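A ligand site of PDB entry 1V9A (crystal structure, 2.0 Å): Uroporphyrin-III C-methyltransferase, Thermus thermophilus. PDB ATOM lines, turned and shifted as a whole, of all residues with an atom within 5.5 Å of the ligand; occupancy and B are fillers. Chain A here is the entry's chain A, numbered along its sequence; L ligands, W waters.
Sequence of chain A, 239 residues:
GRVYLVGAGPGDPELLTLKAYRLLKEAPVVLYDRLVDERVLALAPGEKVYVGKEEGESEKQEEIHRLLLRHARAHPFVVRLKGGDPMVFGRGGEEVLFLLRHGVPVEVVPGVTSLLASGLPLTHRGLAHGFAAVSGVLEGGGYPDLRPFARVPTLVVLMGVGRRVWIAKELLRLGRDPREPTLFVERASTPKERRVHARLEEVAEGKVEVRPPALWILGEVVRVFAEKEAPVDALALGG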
ATOM      1  N   PRO A  10     -16.217 -27.345 -35.308  1.00  0.00           N
ATOM      2  CA  PRO A  10     -16.914 -26.155 -34.805  1.00  0.00           C
ATOM      3  C   PRO A  10     -17.477 -25.163 -35.845  1.00  0.00           C
ATOM      4  O   PRO A  10     -18.252 -24.276 -35.475  1.00  0.00           O
ATOM      5  CB  PRO A  10     -15.862 -25.514 -33.899  1.00  0.00           C
ATOM      6  CG  PRO A  10     -14.600 -25.821 -34.600  1.00  0.00           C
ATOM      7  CD  PRO A  10     -14.774 -27.274 -35.014  1.00  0.00           C
ATOM      8  N   GLY A  11     -17.130 -25.313 -37.116  1.00  0.00           N
ATOM      9  CA  GLY A  11     -17.651 -24.395 -38.129  1.00  0.00           C
ATOM     10  C   GLY A  11     -16.738 -24.168 -39.324  1.00  0.00           C
ATOM     11  O   GLY A  11     -17.167 -24.295 -40.465  1.00  0.00           O
ATOM     12  N   LEU A  35     -26.706 -26.347 -36.017  1.00  0.00           N
ATOM     13  CA  LEU A  35     -25.404 -25.784 -35.660  1.00  0.00           C
ATOM     14  C   LEU A  35     -24.260 -26.369 -36.473  1.00  0.00           C
ATOM     15  O   LEU A  35     -23.095 -26.353 -36.051  1.00  0.00           O
ATOM     16  CB  LEU A  35     -25.114 -25.963 -34.155  1.00  0.00           C
ATOM     17  CG  LEU A  35     -25.944 -25.075 -33.235  1.00  0.00           C
ATOM     18  CD1 LEU A  35     -25.609 -25.409 -31.797  1.00  0.00           C
ATOM     19  CD2 LEU A  35     -25.670 -23.615 -33.542  1.00  0.00           C
ATOM     20  N   GLY A  83     -22.550 -31.265 -35.355  1.00  0.00           N
ATOM     21  CA  GLY A  83     -21.558 -30.236 -35.070  1.00  0.00           C
ATOM     22  C   GLY A  83     -20.514 -30.670 -34.064  1.00  0.00           C
ATOM     23  O   GLY A  83     -20.799 -31.463 -33.163  1.00  0.00           O
ATOM     24  N   GLY A  84     -19.280 -30.180 -34.237  1.00  0.00           N
ATOM     25  CA  GLY A  84     -18.194 -30.518 -33.344  1.00  0.00           C
ATOM     26  C   GLY A  84     -17.863 -31.992 -33.460  1.00  0.00           C
ATOM     27  O   GLY A  84     -17.569 -32.477 -34.560  1.00  0.00           O
ATOM     28  N   ASP A  85     -17.865 -32.692 -32.331  1.00  0.00           N
ATOM     29  CA  ASP A  85     -17.622 -34.127 -32.291  1.00  0.00           C
ATOM     30  C   ASP A  85     -18.997 -34.724 -32.017  1.00  0.00           C
ATOM     31  O   ASP A  85     -19.707 -34.262 -31.145  1.00  0.00           O
ATOM     32  CB  ASP A  85     -16.675 -34.507 -31.174  1.00  0.00           C
ATOM     33  CG  ASP A  85     -16.455 -36.025 -31.095  1.00  0.00           C
ATOM     34  OD1 ASP A  85     -17.264 -36.740 -30.442  1.00  0.00           O
ATOM     35  OD2 ASP A  85     -15.490 -36.499 -31.712  1.00  0.00           O
ATOM     36  N   PRO A  86     -19.357 -35.785 -32.741  1.00  0.00           N
ATOM     37  CA  PRO A  86     -20.671 -36.420 -32.564  1.00  0.00           C
ATOM     38  C   PRO A  86     -20.994 -37.063 -31.228  1.00  0.00           C
ATOM     39  O   PRO A  86     -22.156 -37.211 -30.876  1.00  0.00           O
ATOM     40  CB  PRO A  86     -20.707 -37.435 -33.698  1.00  0.00           C
ATOM     41  CG  PRO A  86     -19.287 -37.876 -33.775  1.00  0.00           C
ATOM     42  CD  PRO A  86     -18.515 -36.564 -33.671  1.00  0.00           C
ATOM     43  N   VAL A  88     -20.295 -36.046 -27.919  1.00  0.00           N
ATOM     44  CA  VAL A  88     -20.426 -35.291 -26.682  1.00  0.00           C
ATOM     45  C   VAL A  88     -21.524 -34.244 -26.837  1.00  0.00           C
ATOM     46  O   VAL A  88     -21.524 -33.474 -27.793  1.00  0.00           O
ATOM     47  CB  VAL A  88     -19.094 -34.621 -26.243  1.00  0.00           C
ATOM     48  CG1 VAL A  88     -18.164 -35.670 -25.618  1.00  0.00           C
ATOM     49  CG2 VAL A  88     -18.403 -33.937 -27.414  1.00  0.00           C
ATOM     50  N   PHE A  89     -22.468 -34.283 -25.906  1.00  0.00           N
ATOM     51  CA  PHE A  89     -23.588 -33.348 -25.857  1.00  0.00           C
ATOM     52  C   PHE A  89     -24.482 -33.262 -27.095  1.00  0.00           C
ATOM     53  O   PHE A  89     -25.137 -32.245 -27.298  1.00  0.00           O
ATOM     54  CB  PHE A  89     -23.066 -31.949 -25.518  1.00  0.00           C
ATOM     55  CG  PHE A  89     -22.200 -31.917 -24.300  1.00  0.00           C
ATOM     56  CD1 PHE A  89     -22.746 -32.069 -23.025  1.00  0.00           C
ATOM     57  CD2 PHE A  89     -20.822 -31.755 -24.418  1.00  0.00           C
ATOM     58  CE1 PHE A  89     -21.937 -32.075 -21.891  1.00  0.00           C
ATOM     59  CE2 PHE A  89     -20.006 -31.758 -23.311  1.00  0.00           C
ATOM     60  CZ  PHE A  89     -20.562 -31.919 -22.033  1.00  0.00           C
ATOM     61  N   GLY A  90     -24.516 -34.293 -27.922  1.00  0.00           N
ATOM     62  CA  GLY A  90     -25.373 -34.234 -29.093  1.00  0.00           C
ATOM     63  C   GLY A  90     -26.352 -35.384 -29.223  1.00  0.00           C
ATOM     64  O   GLY A  90     -27.008 -35.508 -30.255  1.00  0.00           O
ATOM     65  N   VAL A 112     -13.407 -32.124 -34.341  1.00  0.00           N
ATOM     66  CA  VAL A 112     -12.898 -31.104 -33.457  1.00  0.00           C
ATOM     67  C   VAL A 112     -14.122 -30.589 -32.707  1.00  0.00           C
ATOM     68  O   VAL A 112     -15.003 -29.985 -33.304  1.00  0.00           O
ATOM     69  CB  VAL A 112     -12.257 -29.939 -34.242  1.00  0.00           C
ATOM     70  CG1 VAL A 112     -11.903 -28.784 -33.299  1.00  0.00           C
ATOM     71  CG2 VAL A 112     -11.020 -30.439 -34.972  1.00  0.00           C
ATOM     72  N   THR A 113     -14.185 -30.856 -31.404  1.00  0.00           N
ATOM     73  CA  THR A 113     -15.305 -30.433 -30.576  1.00  0.00           C
ATOM     74  C   THR A 113     -15.229 -28.928 -30.285  1.00  0.00           C
ATOM     75  O   THR A 113     -14.148 -28.362 -30.191  1.00  0.00           O
ATOM     76  CB  THR A 113     -15.331 -31.233 -29.241  1.00  0.00           C
ATOM     77  OG1 THR A 113     -16.383 -30.724 -28.395  1.00  0.00           O
ATOM     78  CG2 THR A 113     -13.987 -31.125 -28.516  1.00  0.00           C
ATOM     79  N   SER A 114     -16.377 -28.263 -30.185  1.00  0.00           N
ATOM     80  CA  SER A 114     -16.350 -26.841 -29.906  1.00  0.00           C
ATOM     81  C   SER A 114     -15.666 -26.558 -28.576  1.00  0.00           C
ATOM     82  O   SER A 114     -15.246 -25.437 -28.330  1.00  0.00           O
ATOM     83  CB  SER A 114     -17.764 -26.238 -29.917  1.00  0.00           C
ATOM     84  OG  SER A 114     -18.525 -26.734 -28.829  1.00  0.00           O
ATOM     85  N   LEU A 115     -15.558 -27.580 -27.730  1.00  0.00           N
ATOM     86  CA  LEU A 115     -14.906 -27.421 -26.426  1.00  0.00           C
ATOM     87  C   LEU A 115     -13.453 -26.962 -26.588  1.00  0.00           C
ATOM     88  O   LEU A 115     -12.864 -26.347 -25.688  1.00  0.00           O
ATOM     89  CB  LEU A 115     -14.878 -28.754 -25.664  1.00  0.00           C
ATOM     90  CG  LEU A 115     -16.200 -29.363 -25.193  1.00  0.00           C
ATOM     91  CD1 LEU A 115     -15.978 -30.801 -24.726  1.00  0.00           C
ATOM     92  CD2 LEU A 115     -16.763 -28.498 -24.059  1.00  0.00           C
ATOM     93  N   VAL A 157     -18.740 -24.989 -20.047  1.00  0.00           N
ATOM     94  CA  VAL A 157     -20.181 -25.171 -20.115  1.00  0.00           C
ATOM     95  C   VAL A 157     -20.670 -24.969 -21.546  1.00  0.00           C
ATOM     96  O   VAL A 157     -20.343 -23.971 -22.184  1.00  0.00           O
ATOM     97  CB  VAL A 157     -20.904 -24.150 -19.178  1.00  0.00           C
ATOM     98  CG1 VAL A 157     -22.408 -24.354 -19.235  1.00  0.00           C
ATOM     99  CG2 VAL A 157     -20.397 -24.306 -17.754  1.00  0.00           C
ATOM    100  N   LEU A 158     -21.425 -25.932 -22.042  1.00  0.00           N
ATOM    101  CA  LEU A 158     -21.998 -25.866 -23.380  1.00  0.00           C
ATOM    102  C   LEU A 158     -23.493 -25.660 -23.203  1.00  0.00           C
ATOM    103  O   LEU A 158     -24.048 -26.022 -22.161  1.00  0.00           O
ATOM    104  CB  LEU A 158     -21.714 -27.153 -24.168  1.00  0.00           C
ATOM    105  CG  LEU A 158     -20.247 -27.447 -24.514  1.00  0.00           C
ATOM    106  CD1 LEU A 158     -20.197 -28.533 -25.594  1.00  0.00           C
ATOM    107  CD2 LEU A 158     -19.569 -26.191 -25.047  1.00  0.00           C
ATOM    108  N   MET A 159     -24.150 -25.080 -24.199  1.00  0.00           N
ATOM    109  CA  MET A 159     -25.589 -24.819 -24.134  1.00  0.00           C
ATOM    110  C   MET A 159     -25.922 -24.092 -22.834  1.00  0.00           C
ATOM    111  O   MET A 159     -26.983 -24.305 -22.249  1.00  0.00           O
ATOM    112  CB  MET A 159     -26.371 -26.135 -24.198  1.00  0.00           C
ATOM    113  CG  MET A 159     -26.474 -26.782 -25.575  1.00  0.00           C
ATOM    114  SD  MET A 159     -27.247 -28.424 -25.509  1.00  0.00           S
ATOM    115  CE  MET A 159     -28.360 -28.380 -26.844  1.00  0.00           C
ATOM    116  N   GLY A 160     -25.010 -23.216 -22.385  1.00  0.00           N
ATOM    117  CA  GLY A 160     -25.252 -22.518 -21.137  1.00  0.00           C
ATOM    118  C   GLY A 160     -25.500 -21.017 -21.224  1.00  0.00           C
ATOM    119  O   GLY A 160     -25.482 -20.333 -20.203  1.00  0.00           O
ATOM    120  N   VAL A 185     -17.132 -17.479 -25.649  1.00  0.00           N
ATOM    121  CA  VAL A 185     -16.677 -17.382 -27.033  1.00  0.00           C
ATOM    122  C   VAL A 185     -17.821 -17.785 -27.921  1.00  0.00           C
ATOM    123  O   VAL A 185     -18.200 -18.960 -27.992  1.00  0.00           O
ATOM    124  CB  VAL A 185     -15.471 -18.308 -27.323  1.00  0.00           C
ATOM    125  CG1 VAL A 185     -15.061 -18.177 -28.781  1.00  0.00           C
ATOM    126  CG2 VAL A 185     -14.308 -17.961 -26.404  1.00  0.00           C
ATOM    127  N   GLU A 186     -18.387 -16.790 -28.602  1.00  0.00           N
ATOM    128  CA  GLU A 186     -19.509 -16.991 -29.498  1.00  0.00           C
ATOM    129  C   GLU A 186     -19.091 -17.382 -30.902  1.00  0.00           C
ATOM    130  O   GLU A 186     -18.195 -16.768 -31.490  1.00  0.00           O
ATOM    131  CB  GLU A 186     -20.335 -15.715 -29.593  1.00  0.00           C
ATOM    132  CG  GLU A 186     -21.094 -15.371 -28.340  1.00  0.00           C
ATOM    133  CD  GLU A 186     -21.681 -13.975 -28.400  1.00  0.00           C
ATOM    134  OE1 GLU A 186     -21.713 -13.401 -29.511  1.00  0.00           O
ATOM    135  OE2 GLU A 186     -22.106 -13.461 -27.332  1.00  0.00           O
ATOM    136  N   ARG A 187     -19.758 -18.396 -31.431  1.00  0.00           N
ATOM    137  CA  ARG A 187     -19.493 -18.873 -32.772  1.00  0.00           C
ATOM    138  C   ARG A 187     -18.005 -18.982 -33.038  1.00  0.00           C
ATOM    139  O   ARG A 187     -17.488 -18.402 -33.984  1.00  0.00           O
ATOM    140  CB  ARG A 187     -20.102 -17.916 -33.782  1.00  0.00           C
ATOM    141  CG  ARG A 187     -21.601 -17.814 -33.666  1.00  0.00           C
ATOM    142  CD  ARG A 187     -22.112 -16.771 -34.607  1.00  0.00           C
ATOM    143  NE  ARG A 187     -23.562 -16.667 -34.559  1.00  0.00           N
ATOM    144  CZ  ARG A 187     -24.271 -15.829 -35.305  1.00  0.00           C
ATOM    145  NH1 ARG A 187     -23.656 -15.027 -36.163  1.00  0.00           N
ATOM    146  NH2 ARG A 187     -25.589 -15.784 -35.183  1.00  0.00           N
ATOM    147  N   ALA A 188     -17.323 -19.737 -32.183  1.00  0.00           N
ATOM    148  CA  ALA A 188     -15.897 -19.931 -32.340  1.00  0.00           C
ATOM    149  C   ALA A 188     -15.597 -20.508 -33.732  1.00  0.00           C
ATOM    150  O   ALA A 188     -16.405 -21.244 -34.311  1.00  0.00           O
ATOM    151  CB  ALA A 188     -15.394 -20.876 -31.253  1.00  0.00           C
ATOM    152  N   SER A 189     -14.414 -20.156 -34.245  1.00  0.00           N
ATOM    153  CA  SER A 189     -13.905 -20.606 -35.535  1.00  0.00           C
ATOM    154  C   SER A 189     -14.709 -20.098 -36.728  1.00  0.00           C
ATOM    155  O   SER A 189     -14.605 -20.642 -37.831  1.00  0.00           O
ATOM    156  CB  SER A 189     -13.820 -22.135 -35.565  1.00  0.00           C
ATOM    157  OG  SER A 189     -14.903 -22.675 -36.281  1.00  0.00           O
ATOM    158  N   THR A 190     -15.495 -19.053 -36.532  1.00  0.00           N
ATOM    159  CA  THR A 190     -16.257 -18.495 -37.630  1.00  0.00           C
ATOM    160  C   THR A 190     -15.881 -17.018 -37.747  1.00  0.00           C
ATOM    161  O   THR A 190     -15.291 -16.447 -36.835  1.00  0.00           O
ATOM    162  CB  THR A 190     -17.784 -18.602 -37.406  1.00  0.00           C
ATOM    163  OG1 THR A 190     -18.230 -17.559 -36.542  1.00  0.00           O
ATOM    164  CG2 THR A 190     -18.153 -19.946 -36.792  1.00  0.00           C
ATOM    165  N   PRO A 213     -24.703 -19.562 -30.550  1.00  0.00           N
ATOM    166  CA  PRO A 213     -24.132 -20.595 -29.680  1.00  0.00           C
ATOM    167  C   PRO A 213     -22.816 -20.105 -29.114  1.00  0.00           C
ATOM    168  O   PRO A 213     -22.049 -19.430 -29.789  1.00  0.00           O
ATOM    169  CB  PRO A 213     -23.928 -21.776 -30.634  1.00  0.00           C
ATOM    170  CG  PRO A 213     -23.602 -21.101 -31.915  1.00  0.00           C
ATOM    171  CD  PRO A 213     -24.615 -19.957 -31.960  1.00  0.00           C
ATOM    172  N   ALA A 214     -22.555 -20.445 -27.864  1.00  0.00           N
ATOM    173  CA  ALA A 214     -21.319 -20.010 -27.250  1.00  0.00           C
ATOM    174  C   ALA A 214     -20.735 -21.064 -26.342  1.00  0.00           C
ATOM    175  O   ALA A 214     -21.418 -21.962 -25.853  1.00  0.00           O
ATOM    176  CB  ALA A 214     -21.535 -18.720 -26.481  1.00  0.00           C
ATOM    177  N   LEU A 215     -19.433 -20.906 -26.136  1.00  0.00           N
ATOM    178  CA  LEU A 215     -18.634 -21.788 -25.319  1.00  0.00           C
ATOM    179  C   LEU A 215     -18.363 -20.988 -24.046  1.00  0.00           C
ATOM    180  O   LEU A 215     -17.984 -19.833 -24.123  1.00  0.00           O
ATOM    181  CB  LEU A 215     -17.335 -22.023 -26.070  1.00  0.00           C
ATOM    182  CG  LEU A 215     -16.272 -22.990 -25.624  1.00  0.00           C
ATOM    183  CD1 LEU A 215     -16.846 -24.393 -25.574  1.00  0.00           C
ATOM    184  CD2 LEU A 215     -15.125 -22.909 -26.630  1.00  0.00           C
HETATM  185  N1  LIG L   1     -21.103 -31.997 -30.163  1.00  0.00           N
HETATM  186  C1  LIG L   1     -20.822 -30.542 -30.226  1.00  0.00           C
HETATM  187  C2  LIG L   1     -21.757 -29.867 -29.139  1.00  0.00           C
HETATM  188  C3  LIG L   1     -23.315 -29.958 -29.428  1.00  0.00           C
HETATM  189  S1  LIG L   1     -24.270 -29.162 -28.123  1.00  0.00           S
HETATM  190  C4  LIG L   1     -19.320 -30.298 -29.983  1.00  0.00           C
HETATM  191  O1  LIG L   1     -18.503 -31.318 -29.760  1.00  0.00           O
HETATM  192  O2  LIG L   1     -18.876 -29.096 -30.010  1.00  0.00           O
HETATM  193  C5  LIG L   1     -24.363 -27.459 -28.864  1.00  0.00           C
HETATM  194  C6  LIG L   1     -23.554 -26.448 -28.086  1.00  0.00           C
HETATM  195  O3  LIG L   1     -22.177 -26.499 -28.501  1.00  0.00           O
HETATM  196  C7  LIG L   1     -23.890 -24.948 -28.232  1.00  0.00           C
HETATM  197  O4  LIG L   1     -24.968 -24.536 -27.365  1.00  0.00           O
HETATM  198  C8  LIG L   1     -22.581 -24.270 -27.865  1.00  0.00           C
HETATM  199  O5  LIG L   1     -22.428 -24.140 -26.436  1.00  0.00           O
HETATM  200  C9  LIG L   1     -21.519 -25.242 -28.416  1.00  0.00           C
HETATM  201  N2  LIG L   1     -21.034 -24.895 -29.734  1.00  0.00           N
HETATM  202  C10 LIG L   1     -21.137 -25.601 -30.934  1.00  0.00           C
HETATM  203  N3  LIG L   1     -20.524 -24.936 -31.921  1.00  0.00           N
HETATM  204  C11 LIG L   1     -20.006 -23.791 -31.354  1.00  0.00           C
HETATM  205  C12 LIG L   1     -19.285 -22.690 -31.831  1.00  0.00           C
HETATM  206  N4  LIG L   1     -18.913 -22.622 -33.121  1.00  0.00           N
HETATM  207  N5  LIG L   1     -18.916 -21.671 -30.969  1.00  0.00           N
HETATM  208  C13 LIG L   1     -19.290 -21.762 -29.659  1.00  0.00           C
HETATM  209  N6  LIG L   1     -20.004 -22.782 -29.086  1.00  0.00           N
HETATM  210  C14 LIG L   1     -20.337 -23.745 -29.986  1.00  0.00           C
HETATM  211  O   HOH W   1     -23.154 -32.501 -31.861  1.00  0.00           O
HETATM  212  O   HOH W   2     -24.698 -22.021 -26.559  1.00  0.00           O
HETATM  213  O   HOH W   3     -21.049 -26.779 -34.285  1.00  0.00           O
HETATM  214  O   HOH W   4     -27.266 -24.754 -28.950  1.00  0.00           O
HETATM  215  O   HOH W   5     -22.671 -27.945 -32.561  1.00  0.00           O
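An oxygen (O5) of the ligand lies within hydrogen-bond range of the backbone carbonyl oxygen of Ala 214 (2.5 Å).
O1 of the ligand lies within hydrogen-bond range of OG1 of Thr 113 (2.6 Å).
The backbone NH (N) of Ser 114 is in hydrogen-bond range of an oxygen (O2) of the ligand (2.6 Å).
The side-chain hydroxyl (OG) of Ser 114 sits at hydrogen-bond distance from an oxygen (O2) of the ligand (2.7 Å).
N of Ala 188 is in hydrogen-bond range of N5 of the ligand (2.8 Å).
The backbone carbonyl oxygen of Ala 188 lies within hydrogen-bond range of a nitrogen (N4) of the ligand (3.1 Å).
The backbone carbonyl oxygen (O) of Val 88 lies within hydrogen-bond range of a nitrogen (N1) of the ligand (2.8 Å).
N of Asp 85 lies within hydrogen-bond range of O1 of the ligand (3.0 Å).
The backbone carbonyl oxygen of Asp 85 sits at hydrogen-bond distance from a nitrogen (N1) of the ligand, 2.8 Å away.
N4 of the ligand lies within hydrogen-bond range of O of Pro 10 (3.0 Å).
An oxygen (O5) of the ligand is in hydrogen-bond range of the backbone NH of Met 159 (3.0 Å).
O of Gly 83 sits at hydrogen-bond distance from N1 of the ligand, 3.1 Å away.
The backbone NH (N) of Arg 187 sits close to a nitrogen (N5) of the ligand.
The side-chain hydroxyl (OG1) of Thr 113 lies close to the backbone NH (N) of Leu 115 (3.3 Å).
N of Arg 187 lies within hydrogen-bond range of O of Pro 213 (3.0 Å).
The side-chain hydroxyl (OG1) of Thr 190 sits at hydrogen-bond distance from the backbone carbonyl oxygen (O) of Arg 187 (2.8 Å).
The backbone carbonyl oxygen (O) of Leu 215 is in hydrogen-bond range of the backbone NH (N) of Val 185 (2.9 Å).
S1 of the ligand lies close to O of Phe 89 (3.3 Å).
Merely in contact with the ligand: Val 185 (3.4 Å), Leu 158 (3.5 Å), Leu 215 (3.5 Å), Gly 84 (3.6 Å), Pro 213 (3.6 Å) and Leu 35 (3.8 Å).
17 residues have an atom within 4 Å of the ligand: Pro 10, Leu 35, Gly 83, Gly 84, Asp 85, Val 88, Phe 89, Thr 113, Ser 114, Leu 158, Met 159, Val 185, Arg 187, Ala 188, Pro 213, Ala 214 and Leu 215.
Water W2 bridges O4 of the ligand (2.7 Å) and N of Ala 214 (3.0 Å).
Water W1 lies within hydrogen-bond range of a nitrogen (N1) of the ligand (2.7 Å) and the backbone carbonyl oxygen of Gly 83 (2.9 Å).
Water W3 bridges O of Leu 35 (2.7 Å) and N3 of the ligand (3.0 Å).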
